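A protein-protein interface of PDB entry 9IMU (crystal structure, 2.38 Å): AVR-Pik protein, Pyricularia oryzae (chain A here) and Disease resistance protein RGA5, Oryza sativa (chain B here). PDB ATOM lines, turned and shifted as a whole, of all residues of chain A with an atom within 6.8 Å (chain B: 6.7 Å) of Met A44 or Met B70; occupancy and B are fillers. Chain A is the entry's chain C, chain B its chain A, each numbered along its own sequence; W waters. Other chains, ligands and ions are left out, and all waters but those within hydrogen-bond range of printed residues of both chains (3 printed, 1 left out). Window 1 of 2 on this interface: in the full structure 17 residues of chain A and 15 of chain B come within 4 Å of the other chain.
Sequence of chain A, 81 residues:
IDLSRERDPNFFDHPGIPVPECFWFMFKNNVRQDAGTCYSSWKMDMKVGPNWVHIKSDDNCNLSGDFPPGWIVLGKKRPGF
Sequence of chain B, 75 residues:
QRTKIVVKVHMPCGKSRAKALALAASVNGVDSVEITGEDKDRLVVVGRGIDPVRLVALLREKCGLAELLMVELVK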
ATOM      1  N   TRP A  24     -17.243 -21.026 -18.565  1.00  0.00           N
ATOM      2  CA  TRP A  24     -16.778 -20.517 -17.283  1.00  0.00           C
ATOM      3  C   TRP A  24     -17.961 -19.982 -16.500  1.00  0.00           C
ATOM      4  O   TRP A  24     -18.959 -19.547 -17.073  1.00  0.00           O
ATOM      5  CB  TRP A  24     -15.722 -19.413 -17.443  1.00  0.00           C
ATOM      6  CG  TRP A  24     -16.153 -18.241 -18.288  1.00  0.00           C
ATOM      7  CD1 TRP A  24     -15.934 -18.082 -19.626  1.00  0.00           C
ATOM      8  CD2 TRP A  24     -16.827 -17.051 -17.852  1.00  0.00           C
ATOM      9  NE1 TRP A  24     -16.443 -16.879 -20.052  1.00  0.00           N
ATOM     10  CE2 TRP A  24     -17.001 -16.229 -18.984  1.00  0.00           C
ATOM     11  CE3 TRP A  24     -17.302 -16.602 -16.619  1.00  0.00           C
ATOM     12  CZ2 TRP A  24     -17.651 -14.991 -18.921  1.00  0.00           C
ATOM     13  CZ3 TRP A  24     -17.929 -15.370 -16.559  1.00  0.00           C
ATOM     14  CH2 TRP A  24     -18.092 -14.579 -17.696  1.00  0.00           C
ATOM     15  N   GLY A  36     -20.029 -17.748 -19.173  1.00  0.00           N
ATOM     16  CA  GLY A  36     -19.695 -17.503 -20.559  1.00  0.00           C
ATOM     17  C   GLY A  36     -18.922 -18.654 -21.150  1.00  0.00           C
ATOM     18  O   GLY A  36     -18.919 -19.764 -20.611  1.00  0.00           O
ATOM     19  N   THR A  37     -18.266 -18.377 -22.273  1.00  0.00           N
ATOM     20  CA  THR A  37     -17.472 -19.369 -22.961  1.00  0.00           C
ATOM     21  C   THR A  37     -16.040 -18.870 -23.046  1.00  0.00           C
ATOM     22  O   THR A  37     -15.781 -17.662 -23.067  1.00  0.00           O
ATOM     23  CB  THR A  37     -18.028 -19.669 -24.377  1.00  0.00           C
ATOM     24  OG1 THR A  37     -18.142 -18.454 -25.110  1.00  0.00           O
ATOM     25  CG2 THR A  37     -19.409 -20.289 -24.327  1.00  0.00           C
ATOM     26  N   CYS A  38     -15.102 -19.802 -23.088  1.00  0.00           N
ATOM     27  CA  CYS A  38     -13.720 -19.422 -23.328  1.00  0.00           C
ATOM     28  C   CYS A  38     -12.996 -20.605 -23.943  1.00  0.00           C
ATOM     29  O   CYS A  38     -13.494 -21.735 -23.957  1.00  0.00           O
ATOM     30  CB  CYS A  38     -13.021 -18.957 -22.042  1.00  0.00           C
ATOM     31  SG  CYS A  38     -12.878 -20.273 -20.805  1.00  0.00           S
ATOM     32  N   TYR A  39     -11.806 -20.339 -24.442  1.00  0.00           N
ATOM     33  CA  TYR A  39     -11.032 -21.403 -25.043  1.00  0.00           C
ATOM     34  C   TYR A  39     -10.360 -22.246 -23.976  1.00  0.00           C
ATOM     35  O   TYR A  39     -10.041 -21.766 -22.884  1.00  0.00           O
ATOM     36  CB  TYR A  39     -10.009 -20.819 -26.002  1.00  0.00           C
ATOM     37  CG  TYR A  39     -10.714 -20.255 -27.200  1.00  0.00           C
ATOM     38  CD1 TYR A  39     -11.240 -21.099 -28.169  1.00  0.00           C
ATOM     39  CD2 TYR A  39     -10.900 -18.889 -27.341  1.00  0.00           C
ATOM     40  CE1 TYR A  39     -11.912 -20.594 -29.268  1.00  0.00           C
ATOM     41  CE2 TYR A  39     -11.561 -18.378 -28.426  1.00  0.00           C
ATOM     42  CZ  TYR A  39     -12.060 -19.234 -29.395  1.00  0.00           C
ATOM     43  OH  TYR A  39     -12.734 -18.732 -30.473  1.00  0.00           O
ATOM     44  N   TRP A  42      -5.644 -22.069 -22.994  1.00  0.00           N
ATOM     45  CA  TRP A  42      -5.610 -20.721 -23.514  1.00  0.00           C
ATOM     46  C   TRP A  42      -5.582 -19.791 -22.328  1.00  0.00           C
ATOM     47  O   TRP A  42      -5.097 -20.157 -21.254  1.00  0.00           O
ATOM     48  CB  TRP A  42      -6.837 -20.446 -24.404  1.00  0.00           C
ATOM     49  CG  TRP A  42      -6.689 -19.310 -25.376  1.00  0.00           C
ATOM     50  CD1 TRP A  42      -7.546 -18.269 -25.547  1.00  0.00           C
ATOM     51  CD2 TRP A  42      -5.613 -19.101 -26.296  1.00  0.00           C
ATOM     52  NE1 TRP A  42      -7.077 -17.419 -26.524  1.00  0.00           N
ATOM     53  CE2 TRP A  42      -5.892 -17.912 -27.002  1.00  0.00           C
ATOM     54  CE3 TRP A  42      -4.441 -19.802 -26.587  1.00  0.00           C
ATOM     55  CZ2 TRP A  42      -5.044 -17.404 -27.970  1.00  0.00           C
ATOM     56  CZ3 TRP A  42      -3.602 -19.307 -27.582  1.00  0.00           C
ATOM     57  CH2 TRP A  42      -3.910 -18.120 -28.259  1.00  0.00           C
ATOM     58  N   LYS A  43      -6.213 -18.638 -22.488  1.00  0.00           N
ATOM     59  CA  LYS A  43      -5.957 -17.497 -21.637  1.00  0.00           C
ATOM     60  C   LYS A  43      -6.913 -16.358 -21.954  1.00  0.00           C
ATOM     61  O   LYS A  43      -7.220 -16.090 -23.114  1.00  0.00           O
ATOM     62  CB  LYS A  43      -4.475 -17.127 -21.803  1.00  0.00           C
ATOM     63  CG  LYS A  43      -4.143 -16.746 -23.235  1.00  0.00           C
ATOM     64  CD  LYS A  43      -2.695 -16.466 -23.465  1.00  0.00           C
ATOM     65  CE  LYS A  43      -2.498 -16.206 -24.946  1.00  0.00           C
ATOM     66  NZ  LYS A  43      -3.179 -14.967 -25.340  1.00  0.00           N
ATOM     67  N   MET A  44      -7.411 -15.700 -20.918  1.00  0.00           N
ATOM     68  CA  MET A  44      -8.270 -14.543 -21.080  1.00  0.00           C
ATOM     69  C   MET A  44      -8.007 -13.578 -19.941  1.00  0.00           C
ATOM     70  O   MET A  44      -7.454 -13.955 -18.903  1.00  0.00           O
ATOM     71  CB  MET A  44      -9.740 -14.952 -21.088  1.00  0.00           C
ATOM     72  CG  MET A  44     -10.128 -15.764 -19.863  1.00  0.00           C
ATOM     73  SD  MET A  44     -11.853 -16.283 -19.963  1.00  0.00           S
ATOM     74  CE  MET A  44     -12.057 -17.298 -18.512  1.00  0.00           C
ATOM     75  N   ASP A  45      -8.409 -12.323 -20.150  1.00  0.00           N
ATOM     76  CA  ASP A  45      -8.501 -11.339 -19.082  1.00  0.00           C
ATOM     77  C   ASP A  45      -9.962 -11.070 -18.766  1.00  0.00           C
ATOM     78  O   ASP A  45     -10.786 -10.914 -19.677  1.00  0.00           O
ATOM     79  CB  ASP A  45      -7.798 -10.048 -19.463  1.00  0.00           C
ATOM     80  CG  ASP A  45      -6.355 -10.283 -19.791  1.00  0.00           C
ATOM     81  OD1 ASP A  45      -5.792 -11.187 -19.138  1.00  0.00           O
ATOM     82  OD2 ASP A  45      -5.800  -9.596 -20.692  1.00  0.00           O
ATOM     83  N   MET A  46     -10.272 -10.998 -17.473  1.00  0.00           N
ATOM     84  CA  MET A  46     -11.645 -10.858 -17.006  1.00  0.00           C
ATOM     85  C   MET A  46     -11.735  -9.958 -15.785  1.00  0.00           C
ATOM     86  O   MET A  46     -10.858  -9.979 -14.920  1.00  0.00           O
ATOM     87  CB  MET A  46     -12.238 -12.209 -16.643  1.00  0.00           C
ATOM     88  CG  MET A  46     -13.738 -12.232 -16.661  1.00  0.00           C
ATOM     89  SD  MET A  46     -14.299 -13.910 -16.309  1.00  0.00           S
ATOM     90  CE  MET A  46     -14.374 -14.500 -18.003  1.00  0.00           C
ATOM     91  N   LYS A  47     -12.824  -9.201 -15.715  1.00  0.00           N
ATOM     92  CA  LYS A  47     -13.170  -8.431 -14.533  1.00  0.00           C
ATOM     93  C   LYS A  47     -13.729  -9.383 -13.479  1.00  0.00           C
ATOM     94  O   LYS A  47     -14.811  -9.958 -13.651  1.00  0.00           O
ATOM     95  CB  LYS A  47     -14.179  -7.355 -14.921  1.00  0.00           C
ATOM     96  CG  LYS A  47     -14.655  -6.414 -13.823  1.00  0.00           C
ATOM     97  CD  LYS A  47     -13.493  -5.608 -13.234  1.00  0.00           C
ATOM     98  CE  LYS A  47     -12.795  -4.723 -14.287  1.00  0.00           C
ATOM     99  NZ  LYS A  47     -13.538  -3.560 -14.898  1.00  0.00           N
ATOM    100  N   TRP A  52      -8.997  -6.739 -12.577  1.00  0.00           N
ATOM    101  CA  TRP A  52      -8.793  -7.275 -13.916  1.00  0.00           C
ATOM    102  C   TRP A  52      -7.813  -8.438 -13.799  1.00  0.00           C
ATOM    103  O   TRP A  52      -6.623  -8.223 -13.555  1.00  0.00           O
ATOM    104  CB  TRP A  52      -8.249  -6.184 -14.837  1.00  0.00           C
ATOM    105  CG  TRP A  52      -8.269  -6.527 -16.296  1.00  0.00           C
ATOM    106  CD1 TRP A  52      -7.189  -6.675 -17.119  1.00  0.00           C
ATOM    107  CD2 TRP A  52      -9.429  -6.703 -17.121  1.00  0.00           C
ATOM    108  NE1 TRP A  52      -7.601  -6.957 -18.395  1.00  0.00           N
ATOM    109  CE2 TRP A  52      -8.971  -6.978 -18.428  1.00  0.00           C
ATOM    110  CE3 TRP A  52     -10.810  -6.670 -16.878  1.00  0.00           C
ATOM    111  CZ2 TRP A  52      -9.844  -7.218 -19.497  1.00  0.00           C
ATOM    112  CZ3 TRP A  52     -11.678  -6.905 -17.930  1.00  0.00           C
ATOM    113  CH2 TRP A  52     -11.189  -7.195 -19.232  1.00  0.00           C
ATOM    114  N   VAL A  53      -8.298  -9.665 -13.989  1.00  0.00           N
ATOM    115  CA  VAL A  53      -7.546 -10.871 -13.648  1.00  0.00           C
ATOM    116  C   VAL A  53      -7.196 -11.651 -14.912  1.00  0.00           C
ATOM    117  O   VAL A  53      -8.075 -11.939 -15.739  1.00  0.00           O
ATOM    118  CB  VAL A  53      -8.333 -11.760 -12.673  1.00  0.00           C
ATOM    119  CG1 VAL A  53      -7.541 -13.040 -12.366  1.00  0.00           C
ATOM    120  CG2 VAL A  53      -8.642 -10.989 -11.391  1.00  0.00           C
ATOM    121  N   HIS A  54      -5.915 -12.014 -15.045  1.00  0.00           N
ATOM    122  CA  HIS A  54      -5.465 -12.878 -16.124  1.00  0.00           C
ATOM    123  C   HIS A  54      -5.705 -14.332 -15.749  1.00  0.00           C
ATOM    124  O   HIS A  54      -5.246 -14.793 -14.694  1.00  0.00           O
ATOM    125  CB  HIS A  54      -3.994 -12.650 -16.423  1.00  0.00           C
ATOM    126  CG  HIS A  54      -3.505 -13.393 -17.628  1.00  0.00           C
ATOM    127  ND1 HIS A  54      -3.810 -13.004 -18.916  1.00  0.00           N
ATOM    128  CD2 HIS A  54      -2.721 -14.490 -17.746  1.00  0.00           C
ATOM    129  CE1 HIS A  54      -3.235 -13.826 -19.774  1.00  0.00           C
ATOM    130  NE2 HIS A  54      -2.574 -14.740 -19.090  1.00  0.00           N
ATOM    131  N   ILE A  55      -6.447 -15.046 -16.602  1.00  0.00           N
ATOM    132  CA  ILE A  55      -6.899 -16.410 -16.336  1.00  0.00           C
ATOM    133  C   ILE A  55      -6.374 -17.341 -17.428  1.00  0.00           C
ATOM    134  O   ILE A  55      -6.560 -17.062 -18.615  1.00  0.00           O
ATOM    135  CB  ILE A  55      -8.442 -16.493 -16.238  1.00  0.00           C
ATOM    136  CG1 ILE A  55      -8.970 -15.514 -15.184  1.00  0.00           C
ATOM    137  CG2 ILE A  55      -8.884 -17.892 -15.880  1.00  0.00           C
ATOM    138  CD1 ILE A  55     -10.469 -15.379 -15.156  1.00  0.00           C
ATOM    139  N   LYS A  56      -5.761 -18.461 -17.019  1.00  0.00           N
ATOM    140  CA  LYS A  56      -5.313 -19.540 -17.895  1.00  0.00           C
ATOM    141  C   LYS A  56      -6.321 -20.678 -17.858  1.00  0.00           C
ATOM    142  O   LYS A  56      -6.849 -21.021 -16.794  1.00  0.00           O
ATOM    143  CB  LYS A  56      -3.976 -20.096 -17.413  1.00  0.00           C
ATOM    144  CG  LYS A  56      -2.874 -19.090 -17.307  1.00  0.00           C
ATOM    145  CD  LYS A  56      -2.471 -18.564 -18.639  1.00  0.00           C
ATOM    146  CE  LYS A  56      -1.304 -17.584 -18.517  1.00  0.00           C
ATOM    147  NZ  LYS A  56      -0.960 -17.038 -19.839  1.00  0.00           N
ATOM    148  N   SER A  57      -6.538 -21.301 -19.005  1.00  0.00           N
ATOM    149  CA  SER A  57      -7.316 -22.521 -19.068  1.00  0.00           C
ATOM    150  C   SER A  57      -6.387 -23.647 -19.476  1.00  0.00           C
ATOM    151  O   SER A  57      -5.538 -23.479 -20.349  1.00  0.00           O
ATOM    152  CB  SER A  57      -8.463 -22.407 -20.066  1.00  0.00           C
ATOM    153  OG  SER A  57      -7.949 -22.150 -21.366  1.00  0.00           O
ATOM    154  N   LEU A  63      -9.576 -23.533 -14.892  1.00  0.00           N
ATOM    155  CA  LEU A  63      -9.189 -22.135 -14.904  1.00  0.00           C
ATOM    156  C   LEU A  63      -8.326 -21.837 -13.691  1.00  0.00           C
ATOM    157  O   LEU A  63      -8.650 -22.247 -12.572  1.00  0.00           O
ATOM    158  CB  LEU A  63     -10.421 -21.234 -14.893  1.00  0.00           C
ATOM    159  CG  LEU A  63     -11.419 -21.548 -15.997  1.00  0.00           C
ATOM    160  CD1 LEU A  63     -12.560 -20.550 -15.997  1.00  0.00           C
ATOM    161  CD2 LEU A  63     -10.693 -21.517 -17.324  1.00  0.00           C
ATOM    162  N   VAL A  73     -13.573 -18.102 -10.501  1.00  0.00           N
ATOM    163  CA  VAL A  73     -14.041 -18.408 -11.841  1.00  0.00           C
ATOM    164  C   VAL A  73     -13.668 -19.864 -12.116  1.00  0.00           C
ATOM    165  O   VAL A  73     -12.493 -20.243 -12.021  1.00  0.00           O
ATOM    166  CB  VAL A  73     -13.435 -17.463 -12.888  1.00  0.00           C
ATOM    167  CG1 VAL A  73     -14.122 -17.648 -14.241  1.00  0.00           C
ATOM    168  CG2 VAL A  73     -13.524 -16.016 -12.421  1.00  0.00           C
ATOM    169  N   LYS B   4     -12.101 -11.199 -28.884  1.00  0.00           N
ATOM    170  CA  LYS B   4     -13.451 -10.973 -28.414  1.00  0.00           C
ATOM    171  C   LYS B   4     -13.373 -10.088 -27.179  1.00  0.00           C
ATOM    172  O   LYS B   4     -12.504 -10.286 -26.319  1.00  0.00           O
ATOM    173  CB  LYS B   4     -14.132 -12.302 -28.106  1.00  0.00           C
ATOM    174  CG  LYS B   4     -15.321 -12.175 -27.199  1.00  0.00           C
ATOM    175  CD  LYS B   4     -16.031 -13.502 -27.041  1.00  0.00           C
ATOM    176  CE  LYS B   4     -15.476 -14.290 -25.857  1.00  0.00           C
ATOM    177  NZ  LYS B   4     -16.205 -15.599 -25.680  1.00  0.00           N
ATOM    178  N   ILE B   5     -14.247  -9.090 -27.114  1.00  0.00           N
ATOM    179  CA  ILE B   5     -14.300  -8.150 -26.003  1.00  0.00           C
ATOM    180  C   ILE B   5     -15.746  -8.052 -25.538  1.00  0.00           C
ATOM    181  O   ILE B   5     -16.642  -7.784 -26.345  1.00  0.00           O
ATOM    182  CB  ILE B   5     -13.782  -6.753 -26.392  1.00  0.00           C
ATOM    183  CG1 ILE B   5     -12.451  -6.814 -27.121  1.00  0.00           C
ATOM    184  CG2 ILE B   5     -13.645  -5.892 -25.185  1.00  0.00           C
ATOM    185  CD1 ILE B   5     -12.130  -5.506 -27.798  1.00  0.00           C
ATOM    186  N   VAL B   6     -15.971  -8.243 -24.242  1.00  0.00           N
ATOM    187  CA  VAL B   6     -17.289  -8.096 -23.637  1.00  0.00           C
ATOM    188  C   VAL B   6     -17.262  -6.847 -22.776  1.00  0.00           C
ATOM    189  O   VAL B   6     -16.410  -6.716 -21.882  1.00  0.00           O
ATOM    190  CB  VAL B   6     -17.676  -9.318 -22.791  1.00  0.00           C
ATOM    191  CG1 VAL B   6     -19.031  -9.096 -22.148  1.00  0.00           C
ATOM    192  CG2 VAL B   6     -17.664 -10.589 -23.631  1.00  0.00           C
ATOM    193  N   VAL B   7     -18.195  -5.937 -23.050  1.00  0.00           N
ATOM    194  CA  VAL B   7     -18.332  -4.661 -22.363  1.00  0.00           C
ATOM    195  C   VAL B   7     -19.713  -4.591 -21.740  1.00  0.00           C
ATOM    196  O   VAL B   7     -20.710  -4.937 -22.385  1.00  0.00           O
ATOM    197  CB  VAL B   7     -18.143  -3.466 -23.317  1.00  0.00           C
ATOM    198  CG1 VAL B   7     -18.128  -2.154 -22.516  1.00  0.00           C
ATOM    199  CG2 VAL B   7     -16.903  -3.638 -24.144  1.00  0.00           C
ATOM    200  N   GLU B  67     -18.038  -0.660 -18.657  1.00  0.00           N
ATOM    201  CA  GLU B  67     -16.882  -1.292 -18.029  1.00  0.00           C
ATOM    202  C   GLU B  67     -16.491  -2.559 -18.780  1.00  0.00           C
ATOM    203  O   GLU B  67     -17.348  -3.347 -19.184  1.00  0.00           O
ATOM    204  CB  GLU B  67     -17.131  -1.602 -16.530  1.00  0.00           C
ATOM    205  CG  GLU B  67     -17.993  -2.826 -16.227  1.00  0.00           C
ATOM    206  CD  GLU B  67     -18.036  -3.191 -14.734  1.00  0.00           C
ATOM    207  OE1 GLU B  67     -16.965  -3.186 -14.080  1.00  0.00           O
ATOM    208  OE2 GLU B  67     -19.147  -3.474 -14.217  1.00  0.00           O
ATOM    209  N   LEU B  68     -15.185  -2.739 -18.972  1.00  0.00           N
ATOM    210  CA  LEU B  68     -14.688  -3.961 -19.579  1.00  0.00           C
ATOM    211  C   LEU B  68     -14.990  -5.160 -18.698  1.00  0.00           C
ATOM    212  O   LEU B  68     -14.744  -5.133 -17.491  1.00  0.00           O
ATOM    213  CB  LEU B  68     -13.192  -3.882 -19.814  1.00  0.00           C
ATOM    214  CG  LEU B  68     -12.809  -3.321 -21.163  1.00  0.00           C
ATOM    215  CD1 LEU B  68     -11.285  -3.193 -21.294  1.00  0.00           C
ATOM    216  CD2 LEU B  68     -13.429  -4.187 -22.240  1.00  0.00           C
ATOM    217  N   LEU B  69     -15.520  -6.219 -19.304  1.00  0.00           N
ATOM    218  CA  LEU B  69     -15.739  -7.475 -18.603  1.00  0.00           C
ATOM    219  C   LEU B  69     -14.766  -8.567 -19.003  1.00  0.00           C
ATOM    220  O   LEU B  69     -14.232  -9.255 -18.130  1.00  0.00           O
ATOM    221  CB  LEU B  69     -17.164  -7.964 -18.817  1.00  0.00           C
ATOM    222  CG  LEU B  69     -18.241  -6.968 -18.361  1.00  0.00           C
ATOM    223  CD1 LEU B  69     -19.645  -7.601 -18.418  1.00  0.00           C
ATOM    224  CD2 LEU B  69     -17.972  -6.460 -16.921  1.00  0.00           C
ATOM    225  N   MET B  70     -14.513  -8.756 -20.293  1.00  0.00           N
ATOM    226  CA  MET B  70     -13.468  -9.694 -20.647  1.00  0.00           C
ATOM    227  C   MET B  70     -12.929  -9.379 -22.026  1.00  0.00           C
ATOM    228  O   MET B  70     -13.596  -8.762 -22.861  1.00  0.00           O
ATOM    229  CB  MET B  70     -13.930 -11.147 -20.553  1.00  0.00           C
ATOM    230  CG  MET B  70     -14.948 -11.592 -21.546  1.00  0.00           C
ATOM    231  SD  MET B  70     -14.976 -13.405 -21.611  1.00  0.00           S
ATOM    232  CE  MET B  70     -13.354 -13.692 -22.203  1.00  0.00           C
ATOM    233  N   VAL B  71     -11.676  -9.761 -22.203  1.00  0.00           N
ATOM    234  CA  VAL B  71     -10.950  -9.671 -23.453  1.00  0.00           C
ATOM    235  C   VAL B  71     -10.337 -11.041 -23.656  1.00  0.00           C
ATOM    236  O   VAL B  71      -9.638 -11.543 -22.769  1.00  0.00           O
ATOM    237  CB  VAL B  71      -9.861  -8.589 -23.404  1.00  0.00           C
ATOM    238  CG1 VAL B  71      -9.025  -8.560 -24.710  1.00  0.00           C
ATOM    239  CG2 VAL B  71     -10.502  -7.225 -23.111  1.00  0.00           C
ATOM    240  N   GLU B  72     -10.637 -11.668 -24.784  1.00  0.00           N
ATOM    241  CA  GLU B  72     -10.097 -12.986 -25.063  1.00  0.00           C
ATOM    242  C   GLU B  72      -9.668 -12.974 -26.503  1.00  0.00           C
ATOM    243  O   GLU B  72     -10.479 -12.752 -27.404  1.00  0.00           O
ATOM    244  CB  GLU B  72     -11.086 -14.124 -24.812  1.00  0.00           C
ATOM    245  CG  GLU B  72     -10.361 -15.487 -24.837  1.00  0.00           C
ATOM    246  CD  GLU B  72     -11.304 -16.704 -24.839  1.00  0.00           C
ATOM    247  OE1 GLU B  72     -10.878 -17.792 -24.366  1.00  0.00           O
ATOM    248  OE2 GLU B  72     -12.465 -16.592 -25.306  1.00  0.00           O
ATOM    249  N   LEU B  73      -8.384 -13.153 -26.697  1.00  0.00           N
ATOM    250  CA  LEU B  73      -7.869 -13.286 -28.025  1.00  0.00           C
ATOM    251  C   LEU B  73      -8.408 -14.599 -28.578  1.00  0.00           C
ATOM    252  O   LEU B  73      -8.638 -15.558 -27.835  1.00  0.00           O
ATOM    253  CB  LEU B  73      -6.357 -13.211 -27.914  1.00  0.00           C
ATOM    254  CG  LEU B  73      -5.327 -12.962 -28.973  1.00  0.00           C
ATOM    255  CD1 LEU B  73      -4.252 -12.233 -28.167  1.00  0.00           C
ATOM    256  CD2 LEU B  73      -4.785 -14.260 -29.551  1.00  0.00           C
HETATM  257  O   HOH W   1      -9.688 -18.813 -22.344  1.00  0.00           O
HETATM  258  O   HOH W   2     -18.266 -15.085 -23.199  1.00  0.00           O
HETATM  259  O   HOH W   3      -6.725 -14.091 -24.558  1.00  0.00           O
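CD1 of Trp A42 touches OE1 of Glu B72, at 3.6 Å.
O of Lys A43 touches CG of Glu B72, at 3.6 Å.
Met A44 touches Met B70 (SD to CE, 3.7 Å).
O of Val B71 touches CA of Met A44, 3.7 Å away.
Met A44 touches Glu B72.
Asp A45 touches Met B70.
Met A46 touches Met B70.
Trp A52 touches Leu B68 (CZ3 to O, 3.6 Å).
Met B70 touches Trp A52.
Val B71 touches Trp A52.
The backbone carbonyl oxygen (O) of Thr A37 lies within hydrogen-bond range of the side-chain amino group (NZ) of Lys B4, at 3.4 Å.
The backbone carbonyl oxygen (O) of Leu B69 lies within hydrogen-bond range of the backbone NH (N) of Lys A47.
The backbone NH of Val B71 lies within hydrogen-bond range of the backbone carbonyl oxygen of Asp A45 (2.9 Å).
The side-chain amino group (NZ) of Lys A47 is in hydrogen-bond range of the backbone carbonyl oxygen (O) of Leu B68.
O of Leu B73 is in hydrogen-bond range of NE1 of Trp A42.
The side-chain carboxylate of Glu B67 lies within salt-bridge range of the side-chain amino group of Lys A47, at 3.5 Å.
The side-chain carboxylate of Glu B72 sits at hydrogen-bond distance from the backbone NH of Tyr A39, at 2.7 Å.
Trp A24 touches none of the printed residues of chain B.
Of chain B, only Met B70 (3.7 Å), Val B71 (3.7 Å) and Glu B72 (3.8 Å) come within 4 Å of Met A44.
Val B6 touches none of the printed residues of chain A.
Of the printed residues of chain A, Glu B67 touches Lys A47 (3.5 Å).
Printed residues of chain A within 4 Å of Leu B69: Met A46 (3.2 Å), Lys A47 (2.8 Å) and Trp A52 (3.5 Å).
Of chain A, only Met A44 (3.7 Å), Asp A45 (3.1 Å), Met A46 (3.8 Å) and Trp A52 (3.7 Å) come within 4 Å of Met B70.
The nearest residue of chain B that does not touch Met A44 is Leu B73 (5.8 Å).
The nearest residue of chain A that does not touch Met B70 is Trp A24 (4.1 Å).
Water W3 bridges the backbone carbonyl oxygen of Lys A43 (2.5 Å) and the backbone NH of Leu B73 (2.9 Å).
Water W1 lies within hydrogen-bond range of OE1 of Glu B72, O of Tyr A39 and N of Lys A43.
Water W2 bridges the side-chain amino group of Lys B4 (3.3 Å) and the backbone NH of Thr A37 (3.4 Å).
Of the 11 printed residues of chain B, 8 touch a printed residue of chain A.
Hydrophobic or aromatic side chains of chain B that line the printed part of chain A: Leu B68, Met B70, Val B71 and Leu B73.
Of the 19 printed residues of chain A, 10 touch a printed residue of chain B.
Hydrophobic or aromatic side chains of chain A within 4 Å of the printed part of chain B: Tyr A39, Trp A42, Met A44, Met A46 and Trp A52.
Among the printed residues, Asp or Glu carboxylates within 4 Å of a Lys or Arg side-chain nitrogen of the other chain: Lys A47 with Glu B67.
ND1 of His A54 is in hydrogen-bond range of OD1 of Asp A45 (2.7 Å).
The side-chain hydroxyl (OG) of Ser A57 sits at hydrogen-bond distance from the backbone carbonyl oxygen (O) of Tyr A39 (2.6 Å).
N of Trp A42 is in hydrogen-bond range of OG of Ser A57.
NZ of Lys B4 is in salt-bridge range of OE2 of Glu B72, 3.9 Å away.
O of Met B70 lies within hydrogen-bond range of N of Val B6 (2.8 Å).
O of Met A46 is in hydrogen-bond range of N of Val A53, 2.7 Å away.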
